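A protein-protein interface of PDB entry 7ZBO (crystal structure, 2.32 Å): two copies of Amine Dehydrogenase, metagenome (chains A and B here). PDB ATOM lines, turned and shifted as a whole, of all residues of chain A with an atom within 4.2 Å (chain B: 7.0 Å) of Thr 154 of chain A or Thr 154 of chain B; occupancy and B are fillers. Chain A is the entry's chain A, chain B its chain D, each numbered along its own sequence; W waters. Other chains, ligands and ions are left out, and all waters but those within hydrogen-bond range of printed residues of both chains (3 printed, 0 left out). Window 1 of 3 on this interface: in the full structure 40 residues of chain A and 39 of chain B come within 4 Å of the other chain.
Water W2 bridges O of Arg 153 of chain A (2.7 Å) and N of Tyr 346 of chain B (2.8 Å). Water W1 bridges O of Ala 157 of chain A (2.7 Å) and O of Glu 344 of chain B (2.9 Å). Water W3 lies within hydrogen-bond range of O of Met 343 of chain B and O of Arg 153 of chain A.
Hydrophobic or aromatic side chains of chain A within 4 Å of the printed part of chain B: Met 151, Met 155, Ala 157 and Met 343. Printed residues of chain B that touch a printed residue of chain A: Met 151, Thr 154, Met 155, Ala 157, Met 158, Thr 342, Met 343, Glu 344 and Tyr 346. Hydrophobic or aromatic side chains of chain B within 4 Å of the printed part of chain A: Met 151, Met 155, Ala 157, Met 158, Met 343 and Tyr 346. Along chain B the printed residues that touch a printed residue of chain A span positions 151 to 346.
The side-chain sulfur of Met 151 of chain A lies within hydrogen-bond range of the backbone NH of Met 155 of chain B, at 3.8 Å. OG1 of Thr 154 of chain A is in hydrogen-bond range of OG1 of Thr 154 of chain B (2.7 Å). The backbone NH (N) of Met 155 of chain A lies within hydrogen-bond range of the side-chain sulfur (SD) of Met 151 of chain B (3.6 Å). The side-chain hydroxyl (OG1) of Thr 342 of chain A sits at hydrogen-bond distance from the side-chain hydroxyl (OG1) of Thr 342 of chain B.
Met 151 of chain A touches Thr 154 of chain B, and with the chains exchanged Thr 154 of chain A touches Met 151 of chain B. Met 151 of chain A touches Met 155 of chain B, and with the chains exchanged Met 155 of chain A touches Met 151 of chain B. Thr 154 of chain A touches its own counterpart, Thr 154 of chain B. Thr 154 of chain A touches Thr 342 of chain B, and with the chains exchanged Thr 342 of chain A touches Thr 154 of chain B. Positions printed for both chains: 150, 151, 152, 153, 154, 155, 156, 157, 342 and 343. Of the 17 pairs that touch across the chains among the printed residues, 13 have their exchanged pair printed and touching as well.
The side-chain carboxylate (OD2) of Asp 150 of chain A lies within hydrogen-bond range of the backbone NH (N) of Met 343 of chain A (3.0 Å). O of Gly 146 of chain B is in hydrogen-bond range of N of Met 151 of chain B (3.2 Å). The backbone NH (N) of Met 343 of chain B is in hydrogen-bond range of the side-chain carboxylate (OD2) of Asp 150 of chain B, 3.0 Å away.
Thr 154 of chain A touches just these residues of chain B: Met 151 (3.6 Å), Thr 154 (2.7 Å), Thr 342 (3.6 Å) and Met 343 (3.8 Å). Printed residues of chain B within 4 Å of Met 155 of chain A: Met 151. Printed residues of chain A within 4 Å of Met 151 of chain B: Met 151, Thr 154 and Met 155. Of chain A, only Met 151, Thr 154, Thr 342 and Met 343 come within 4 Å of Thr 154 of chain B. Of the printed residues of chain A, Met 155 of chain B touches Met 151. Of the printed residues of chain A, Met 343 of chain B touches Thr 154 and Ala 157. The nearest residue of chain B that does not touch Thr 154 of chain A is Asp 150 of chain B (4.2 Å). The nearest printed residue of chain A that does not touch Thr 154 of chain B is Asp 150 of chain A (4.2 Å).
Among the printed residues, merely in contact across the chains: Met 151 of chain A with Met 151 of chain B, Met 151 of chain A with Thr 154 of chain B, Thr 154 of chain A with Met 151 of chain B, Thr 154 of chain A with Thr 342 of chain B, Thr 154 of chain A with Met 343 of chain B, Ala 156 of chain A with Tyr 346 of chain B, Ala 157 of chain A with Met 343 of chain B, Ala 157 of chain A with Glu 344 of chain B, Ala 157 of chain A with Tyr 346 of chain B, Thr 342 of chain A with Thr 154 of chain B, Met 343 of chain A with Thr 154 of chain B, Met 343 of chain A with Ala 157 of chain B and Met 343 of chain A with Met 158 of chain B.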
ATOM      1  N   ASP A 150       8.690 -11.154   6.719  1.00  0.00           N
ATOM      2  CA  ASP A 150       9.120  -9.740   6.864  1.00  0.00           C
ATOM      3  C   ASP A 150       8.169  -8.793   6.119  1.00  0.00           C
ATOM      4  O   ASP A 150       7.796  -7.765   6.704  1.00  0.00           O
ATOM      5  CB  ASP A 150      10.561  -9.534   6.417  1.00  0.00           C
ATOM      6  CG  ASP A 150      11.263  -8.473   7.252  1.00  0.00           C
ATOM      7  OD1 ASP A 150      10.659  -7.978   8.226  1.00  0.00           O
ATOM      8  OD2 ASP A 150      12.382  -8.136   6.904  1.00  0.00           O
ATOM      9  N   MET A 151       7.763  -9.122   4.890  1.00  0.00           N
ATOM     10  CA  MET A 151       6.727  -8.363   4.154  1.00  0.00           C
ATOM     11  C   MET A 151       5.481  -8.250   5.040  1.00  0.00           C
ATOM     12  O   MET A 151       4.998  -7.114   5.224  1.00  0.00           O
ATOM     13  CB  MET A 151       6.350  -9.035   2.829  1.00  0.00           C
ATOM     14  CG  MET A 151       7.365  -8.822   1.756  1.00  0.00           C
ATOM     15  SD  MET A 151       7.335  -7.117   1.144  1.00  0.00           S
ATOM     16  CE  MET A 151       5.790  -7.116   0.244  1.00  0.00           C
ATOM     17  N   ALA A 152       4.993  -9.351   5.614  1.00  0.00           N
ATOM     18  CA  ALA A 152       3.784  -9.330   6.470  1.00  0.00           C
ATOM     19  C   ALA A 152       4.051  -8.543   7.745  1.00  0.00           C
ATOM     20  O   ALA A 152       3.096  -7.919   8.254  1.00  0.00           O
ATOM     21  CB  ALA A 152       3.324 -10.725   6.787  1.00  0.00           C
ATOM     22  N   ARG A 153       5.293  -8.535   8.233  1.00  0.00           N
ATOM     23  CA  ARG A 153       5.617  -7.816   9.498  1.00  0.00           C
ATOM     24  C   ARG A 153       5.472  -6.308   9.269  1.00  0.00           C
ATOM     25  O   ARG A 153       5.016  -5.615  10.194  1.00  0.00           O
ATOM     26  CB  ARG A 153       7.029  -8.114   9.999  1.00  0.00           C
ATOM     27  CG  ARG A 153       7.375  -7.322  11.260  1.00  0.00           C
ATOM     28  CD  ARG A 153       8.670  -7.780  11.922  1.00  0.00           C
ATOM     29  NE  ARG A 153       9.806  -7.775  11.014  1.00  0.00           N
ATOM     30  CZ  ARG A 153      11.058  -7.729  11.393  1.00  0.00           C
ATOM     31  NH1 ARG A 153      11.351  -7.734  12.678  1.00  0.00           N
ATOM     32  NH2 ARG A 153      12.021  -7.706  10.483  1.00  0.00           N
ATOM     33  N   THR A 154       5.885  -5.813   8.094  1.00  0.00           N
ATOM     34  CA  THR A 154       5.717  -4.391   7.702  1.00  0.00           C
ATOM     35  C   THR A 154       4.211  -4.098   7.657  1.00  0.00           C
ATOM     36  O   THR A 154       3.749  -3.190   8.382  1.00  0.00           O
ATOM     37  CB  THR A 154       6.399  -4.101   6.365  1.00  0.00           C
ATOM     38  OG1 THR A 154       7.804  -4.246   6.468  1.00  0.00           O
ATOM     39  CG2 THR A 154       6.129  -2.702   5.883  1.00  0.00           C
ATOM     40  N   MET A 155       3.471  -4.869   6.854  1.00  0.00           N
ATOM     41  CA  MET A 155       2.018  -4.690   6.656  1.00  0.00           C
ATOM     42  C   MET A 155       1.308  -4.704   8.012  1.00  0.00           C
ATOM     43  O   MET A 155       0.400  -3.900   8.194  1.00  0.00           O
ATOM     44  CB  MET A 155       1.419  -5.781   5.763  1.00  0.00           C
ATOM     45  CG  MET A 155       0.036  -5.428   5.274  1.00  0.00           C
ATOM     46  SD  MET A 155      -0.653  -6.582   4.064  1.00  0.00           S
ATOM     47  CE  MET A 155      -0.744  -8.081   5.039  1.00  0.00           C
ATOM     48  N   ALA A 156       1.698  -5.562   8.944  1.00  0.00           N
ATOM     49  CA  ALA A 156       0.961  -5.757  10.208  1.00  0.00           C
ATOM     50  C   ALA A 156       1.111  -4.548  11.146  1.00  0.00           C
ATOM     51  O   ALA A 156       0.261  -4.420  12.024  1.00  0.00           O
ATOM     52  CB  ALA A 156       1.409  -7.027  10.876  1.00  0.00           C
ATOM     53  N   ALA A 157       2.130  -3.690  10.972  1.00  0.00           N
ATOM     54  CA  ALA A 157       2.301  -2.442  11.755  1.00  0.00           C
ATOM     55  C   ALA A 157       1.037  -1.583  11.613  1.00  0.00           C
ATOM     56  O   ALA A 157       0.749  -0.786  12.539  1.00  0.00           O
ATOM     57  CB  ALA A 157       3.514  -1.678  11.271  1.00  0.00           C
ATOM     58  N   THR A 342      13.962  -4.787   9.548  1.00  0.00           N
ATOM     59  CA  THR A 342      13.619  -5.149   8.139  1.00  0.00           C
ATOM     60  C   THR A 342      14.899  -5.520   7.365  1.00  0.00           C
ATOM     61  O   THR A 342      15.999  -5.032   7.723  1.00  0.00           O
ATOM     62  CB  THR A 342      12.852  -4.004   7.463  1.00  0.00           C
ATOM     63  OG1 THR A 342      11.766  -3.663   8.327  1.00  0.00           O
ATOM     64  CG2 THR A 342      12.344  -4.347   6.078  1.00  0.00           C
ATOM     65  N   MET A 343      14.775  -6.370   6.351  1.00  0.00           N
ATOM     66  CA  MET A 343      15.859  -6.639   5.364  1.00  0.00           C
ATOM     67  C   MET A 343      16.519  -5.300   5.009  1.00  0.00           C
ATOM     68  O   MET A 343      15.784  -4.380   4.725  1.00  0.00           O
ATOM     69  CB  MET A 343      15.283  -7.274   4.099  1.00  0.00           C
ATOM     70  CG  MET A 343      14.701  -8.654   4.307  1.00  0.00           C
ATOM     71  SD  MET A 343      13.994  -9.322   2.762  1.00  0.00           S
ATOM     72  CE  MET A 343      12.372  -8.546   2.779  1.00  0.00           C
ATOM     73  N   GLY B 146       3.140   4.773   4.602  1.00  0.00           N
ATOM     74  CA  GLY B 146       3.215   3.406   5.141  1.00  0.00           C
ATOM     75  C   GLY B 146       2.824   2.355   4.108  1.00  0.00           C
ATOM     76  O   GLY B 146       3.619   1.418   3.897  1.00  0.00           O
ATOM     77  N   CYS B 149       4.929   3.579   0.136  1.00  0.00           N
ATOM     78  CA  CYS B 149       6.402   3.755   0.171  1.00  0.00           C
ATOM     79  C   CYS B 149       7.072   2.711   1.073  1.00  0.00           C
ATOM     80  O   CYS B 149       8.029   2.037   0.584  1.00  0.00           O
ATOM     81  CB  CYS B 149       6.747   5.190   0.553  1.00  0.00           C
ATOM     82  SG  CYS B 149       6.330   6.351  -0.788  1.00  0.00           S
ATOM     83  N   ASP B 150       6.632   2.564   2.332  1.00  0.00           N
ATOM     84  CA  ASP B 150       7.317   1.675   3.309  1.00  0.00           C
ATOM     85  C   ASP B 150       7.150   0.197   2.899  1.00  0.00           C
ATOM     86  O   ASP B 150       8.132  -0.543   2.958  1.00  0.00           O
ATOM     87  CB  ASP B 150       6.813   1.899   4.723  1.00  0.00           C
ATOM     88  CG  ASP B 150       7.900   1.703   5.760  1.00  0.00           C
ATOM     89  OD1 ASP B 150       9.063   1.455   5.341  1.00  0.00           O
ATOM     90  OD2 ASP B 150       7.602   1.919   6.978  1.00  0.00           O
ATOM     91  N   MET B 151       5.953  -0.226   2.476  1.00  0.00           N
ATOM     92  CA  MET B 151       5.742  -1.589   1.919  1.00  0.00           C
ATOM     93  C   MET B 151       6.738  -1.823   0.772  1.00  0.00           C
ATOM     94  O   MET B 151       7.423  -2.824   0.798  1.00  0.00           O
ATOM     95  CB  MET B 151       4.316  -1.779   1.424  1.00  0.00           C
ATOM     96  CG  MET B 151       3.339  -1.992   2.566  1.00  0.00           C
ATOM     97  SD  MET B 151       3.546  -3.557   3.506  1.00  0.00           S
ATOM     98  CE  MET B 151       3.270  -4.739   2.191  1.00  0.00           C
ATOM     99  N   ALA B 152       6.871  -0.899  -0.173  1.00  0.00           N
ATOM    100  CA  ALA B 152       7.788  -1.056  -1.335  1.00  0.00           C
ATOM    101  C   ALA B 152       9.232  -1.003  -0.852  1.00  0.00           C
ATOM    102  O   ALA B 152      10.079  -1.691  -1.481  1.00  0.00           O
ATOM    103  CB  ALA B 152       7.526  -0.031  -2.393  1.00  0.00           C
ATOM    104  N   ARG B 153       9.524  -0.296   0.243  1.00  0.00           N
ATOM    105  CA  ARG B 153      10.914  -0.206   0.769  1.00  0.00           C
ATOM    106  C   ARG B 153      11.351  -1.577   1.263  1.00  0.00           C
ATOM    107  O   ARG B 153      12.523  -1.933   1.055  1.00  0.00           O
ATOM    108  CB  ARG B 153      11.060   0.826   1.898  1.00  0.00           C
ATOM    109  CG  ARG B 153      12.451   0.846   2.514  1.00  0.00           C
ATOM    110  CD  ARG B 153      12.701   2.056   3.405  1.00  0.00           C
ATOM    111  NE  ARG B 153      11.748   2.166   4.496  1.00  0.00           N
ATOM    112  CZ  ARG B 153      11.926   2.921   5.558  1.00  0.00           C
ATOM    113  NH1 ARG B 153      13.002   3.694   5.664  1.00  0.00           N
ATOM    114  NH2 ARG B 153      11.013   2.917   6.510  1.00  0.00           N
ATOM    115  N   THR B 154      10.460  -2.306   1.938  1.00  0.00           N
ATOM    116  CA  THR B 154      10.699  -3.685   2.425  1.00  0.00           C
ATOM    117  C   THR B 154      10.937  -4.562   1.186  1.00  0.00           C
ATOM    118  O   THR B 154      12.008  -5.201   1.100  1.00  0.00           O
ATOM    119  CB  THR B 154       9.512  -4.172   3.267  1.00  0.00           C
ATOM    120  OG1 THR B 154       9.457  -3.422   4.486  1.00  0.00           O
ATOM    121  CG2 THR B 154       9.570  -5.652   3.577  1.00  0.00           C
ATOM    122  N   MET B 155       9.983  -4.575   0.254  1.00  0.00           N
ATOM    123  CA  MET B 155      10.036  -5.425  -0.958  1.00  0.00           C
ATOM    124  C   MET B 155      11.337  -5.158  -1.715  1.00  0.00           C
ATOM    125  O   MET B 155      11.961  -6.137  -2.165  1.00  0.00           O
ATOM    126  CB  MET B 155       8.850  -5.187  -1.894  1.00  0.00           C
ATOM    127  CG  MET B 155       8.727  -6.299  -2.950  1.00  0.00           C
ATOM    128  SD  MET B 155       7.217  -6.177  -3.987  1.00  0.00           S
ATOM    129  CE  MET B 155       7.475  -4.577  -4.769  1.00  0.00           C
ATOM    130  N   ALA B 156      11.771  -3.904  -1.822  1.00  0.00           N
ATOM    131  CA  ALA B 156      12.930  -3.547  -2.682  1.00  0.00           C
ATOM    132  C   ALA B 156      14.252  -4.045  -2.084  1.00  0.00           C
ATOM    133  O   ALA B 156      15.202  -4.143  -2.855  1.00  0.00           O
ATOM    134  CB  ALA B 156      12.967  -2.058  -2.919  1.00  0.00           C
ATOM    135  N   ALA B 157      14.333  -4.349  -0.777  1.00  0.00           N
ATOM    136  CA  ALA B 157      15.536  -4.932  -0.142  1.00  0.00           C
ATOM    137  C   ALA B 157      15.920  -6.224  -0.876  1.00  0.00           C
ATOM    138  O   ALA B 157      17.088  -6.604  -0.859  1.00  0.00           O
ATOM    139  CB  ALA B 157      15.285  -5.186   1.328  1.00  0.00           C
ATOM    140  N   MET B 158      14.946  -6.874  -1.506  1.00  0.00           N
ATOM    141  CA  MET B 158      15.103  -8.201  -2.152  1.00  0.00           C
ATOM    142  C   MET B 158      15.509  -8.005  -3.612  1.00  0.00           C
ATOM    143  O   MET B 158      15.557  -9.012  -4.357  1.00  0.00           O
ATOM    144  CB  MET B 158      13.809  -9.027  -2.071  1.00  0.00           C
ATOM    145  CG  MET B 158      13.393  -9.322  -0.649  1.00  0.00           C
ATOM    146  SD  MET B 158      11.956 -10.385  -0.499  1.00  0.00           S
ATOM    147  CE  MET B 158      10.655  -9.257  -0.990  1.00  0.00           C
ATOM    148  N   MET B 159      15.834  -6.777  -4.013  1.00  0.00           N
ATOM    149  CA  MET B 159      16.375  -6.504  -5.369  1.00  0.00           C
ATOM    150  C   MET B 159      17.903  -6.391  -5.285  1.00  0.00           C
ATOM    151  O   MET B 159      18.405  -5.789  -4.312  1.00  0.00           O
ATOM    152  CB  MET B 159      15.773  -5.222  -5.946  1.00  0.00           C
ATOM    153  CG  MET B 159      14.284  -5.290  -6.128  1.00  0.00           C
ATOM    154  SD  MET B 159      13.810  -6.571  -7.304  1.00  0.00           S
ATOM    155  CE  MET B 159      14.221  -5.755  -8.851  1.00  0.00           C
ATOM    156  N   LEU B 295       8.890  -4.007  -9.299  1.00  0.00           N
ATOM    157  CA  LEU B 295      10.316  -3.669  -9.470  1.00  0.00           C
ATOM    158  C   LEU B 295      10.826  -4.478 -10.663  1.00  0.00           C
ATOM    159  O   LEU B 295      10.623  -5.684 -10.685  1.00  0.00           O
ATOM    160  CB  LEU B 295      11.065  -3.937  -8.158  1.00  0.00           C
ATOM    161  CG  LEU B 295      10.431  -3.297  -6.917  1.00  0.00           C
ATOM    162  CD1 LEU B 295      11.033  -3.841  -5.631  1.00  0.00           C
ATOM    163  CD2 LEU B 295      10.549  -1.783  -6.953  1.00  0.00           C
ATOM    164  N   THR B 342      11.207   1.042   9.621  1.00  0.00           N
ATOM    165  CA  THR B 342       9.836   0.576   9.273  1.00  0.00           C
ATOM    166  C   THR B 342       8.835   1.063  10.333  1.00  0.00           C
ATOM    167  O   THR B 342       9.246   1.306  11.491  1.00  0.00           O
ATOM    168  CB  THR B 342       9.813  -0.945   9.083  1.00  0.00           C
ATOM    169  OG1 THR B 342      10.759  -1.228   8.057  1.00  0.00           O
ATOM    170  CG2 THR B 342       8.479  -1.479   8.609  1.00  0.00           C
ATOM    171  N   MET B 343       7.574   1.244   9.935  1.00  0.00           N
ATOM    172  CA  MET B 343       6.445   1.499  10.867  1.00  0.00           C
ATOM    173  C   MET B 343       6.620   0.593  12.083  1.00  0.00           C
ATOM    174  O   MET B 343       6.879  -0.600  11.859  1.00  0.00           O
ATOM    175  CB  MET B 343       5.103   1.183  10.196  1.00  0.00           C
ATOM    176  CG  MET B 343       4.754   2.084   9.046  1.00  0.00           C
ATOM    177  SD  MET B 343       3.182   1.612   8.254  1.00  0.00           S
ATOM    178  CE  MET B 343       3.787   0.369   7.134  1.00  0.00           C
ATOM    179  N   GLU B 344       6.461   1.104  13.301  1.00  0.00           N
ATOM    180  CA  GLU B 344       6.563   0.297  14.546  1.00  0.00           C
ATOM    181  C   GLU B 344       5.684  -0.966  14.443  1.00  0.00           C
ATOM    182  O   GLU B 344       4.475  -0.836  14.143  1.00  0.00           O
ATOM    183  CB  GLU B 344       6.162   1.137  15.754  1.00  0.00           C
ATOM    184  CG  GLU B 344       6.598   0.555  17.086  1.00  0.00           C
ATOM    185  CD  GLU B 344       8.083   0.240  17.205  1.00  0.00           C
ATOM    186  OE1 GLU B 344       8.405  -0.909  17.571  1.00  0.00           O
ATOM    187  OE2 GLU B 344       8.920   1.124  16.908  1.00  0.00           O
ATOM    188  N   ALA B 345       6.283  -2.146  14.686  1.00  0.00           N
ATOM    189  CA  ALA B 345       5.674  -3.492  14.507  1.00  0.00           C
ATOM    190  C   ALA B 345       4.425  -3.663  15.381  1.00  0.00           C
ATOM    191  O   ALA B 345       4.388  -3.110  16.494  1.00  0.00           O
ATOM    192  CB  ALA B 345       6.679  -4.565  14.821  1.00  0.00           C
ATOM    193  N   TYR B 346       3.424  -4.387  14.869  1.00  0.00           N
ATOM    194  CA  TYR B 346       2.242  -4.818  15.651  1.00  0.00           C
ATOM    195  C   TYR B 346       2.723  -5.735  16.770  1.00  0.00           C
ATOM    196  O   TYR B 346       3.560  -6.592  16.533  1.00  0.00           O
ATOM    197  CB  TYR B 346       1.189  -5.572  14.835  1.00  0.00           C
ATOM    198  CG  TYR B 346       0.034  -6.024  15.694  1.00  0.00           C
ATOM    199  CD1 TYR B 346      -0.950  -5.134  16.079  1.00  0.00           C
ATOM    200  CD2 TYR B 346      -0.047  -7.308  16.193  1.00  0.00           C
ATOM    201  CE1 TYR B 346      -2.003  -5.516  16.897  1.00  0.00           C
ATOM    202  CE2 TYR B 346      -1.096  -7.705  17.015  1.00  0.00           C
ATOM    203  CZ  TYR B 346      -2.086  -6.809  17.360  1.00  0.00           C
ATOM    204  OH  TYR B 346      -3.117  -7.176  18.171  1.00  0.00           O
HETATM  205  O   HOH W   1       1.724  -1.133  15.064  1.00  0.00           O
HETATM  206  O   HOH W   2       4.300  -6.080  12.752  1.00  0.00           O
HETATM  207  O   HOH W   3       6.899  -3.546  11.421  1.00  0.00           O
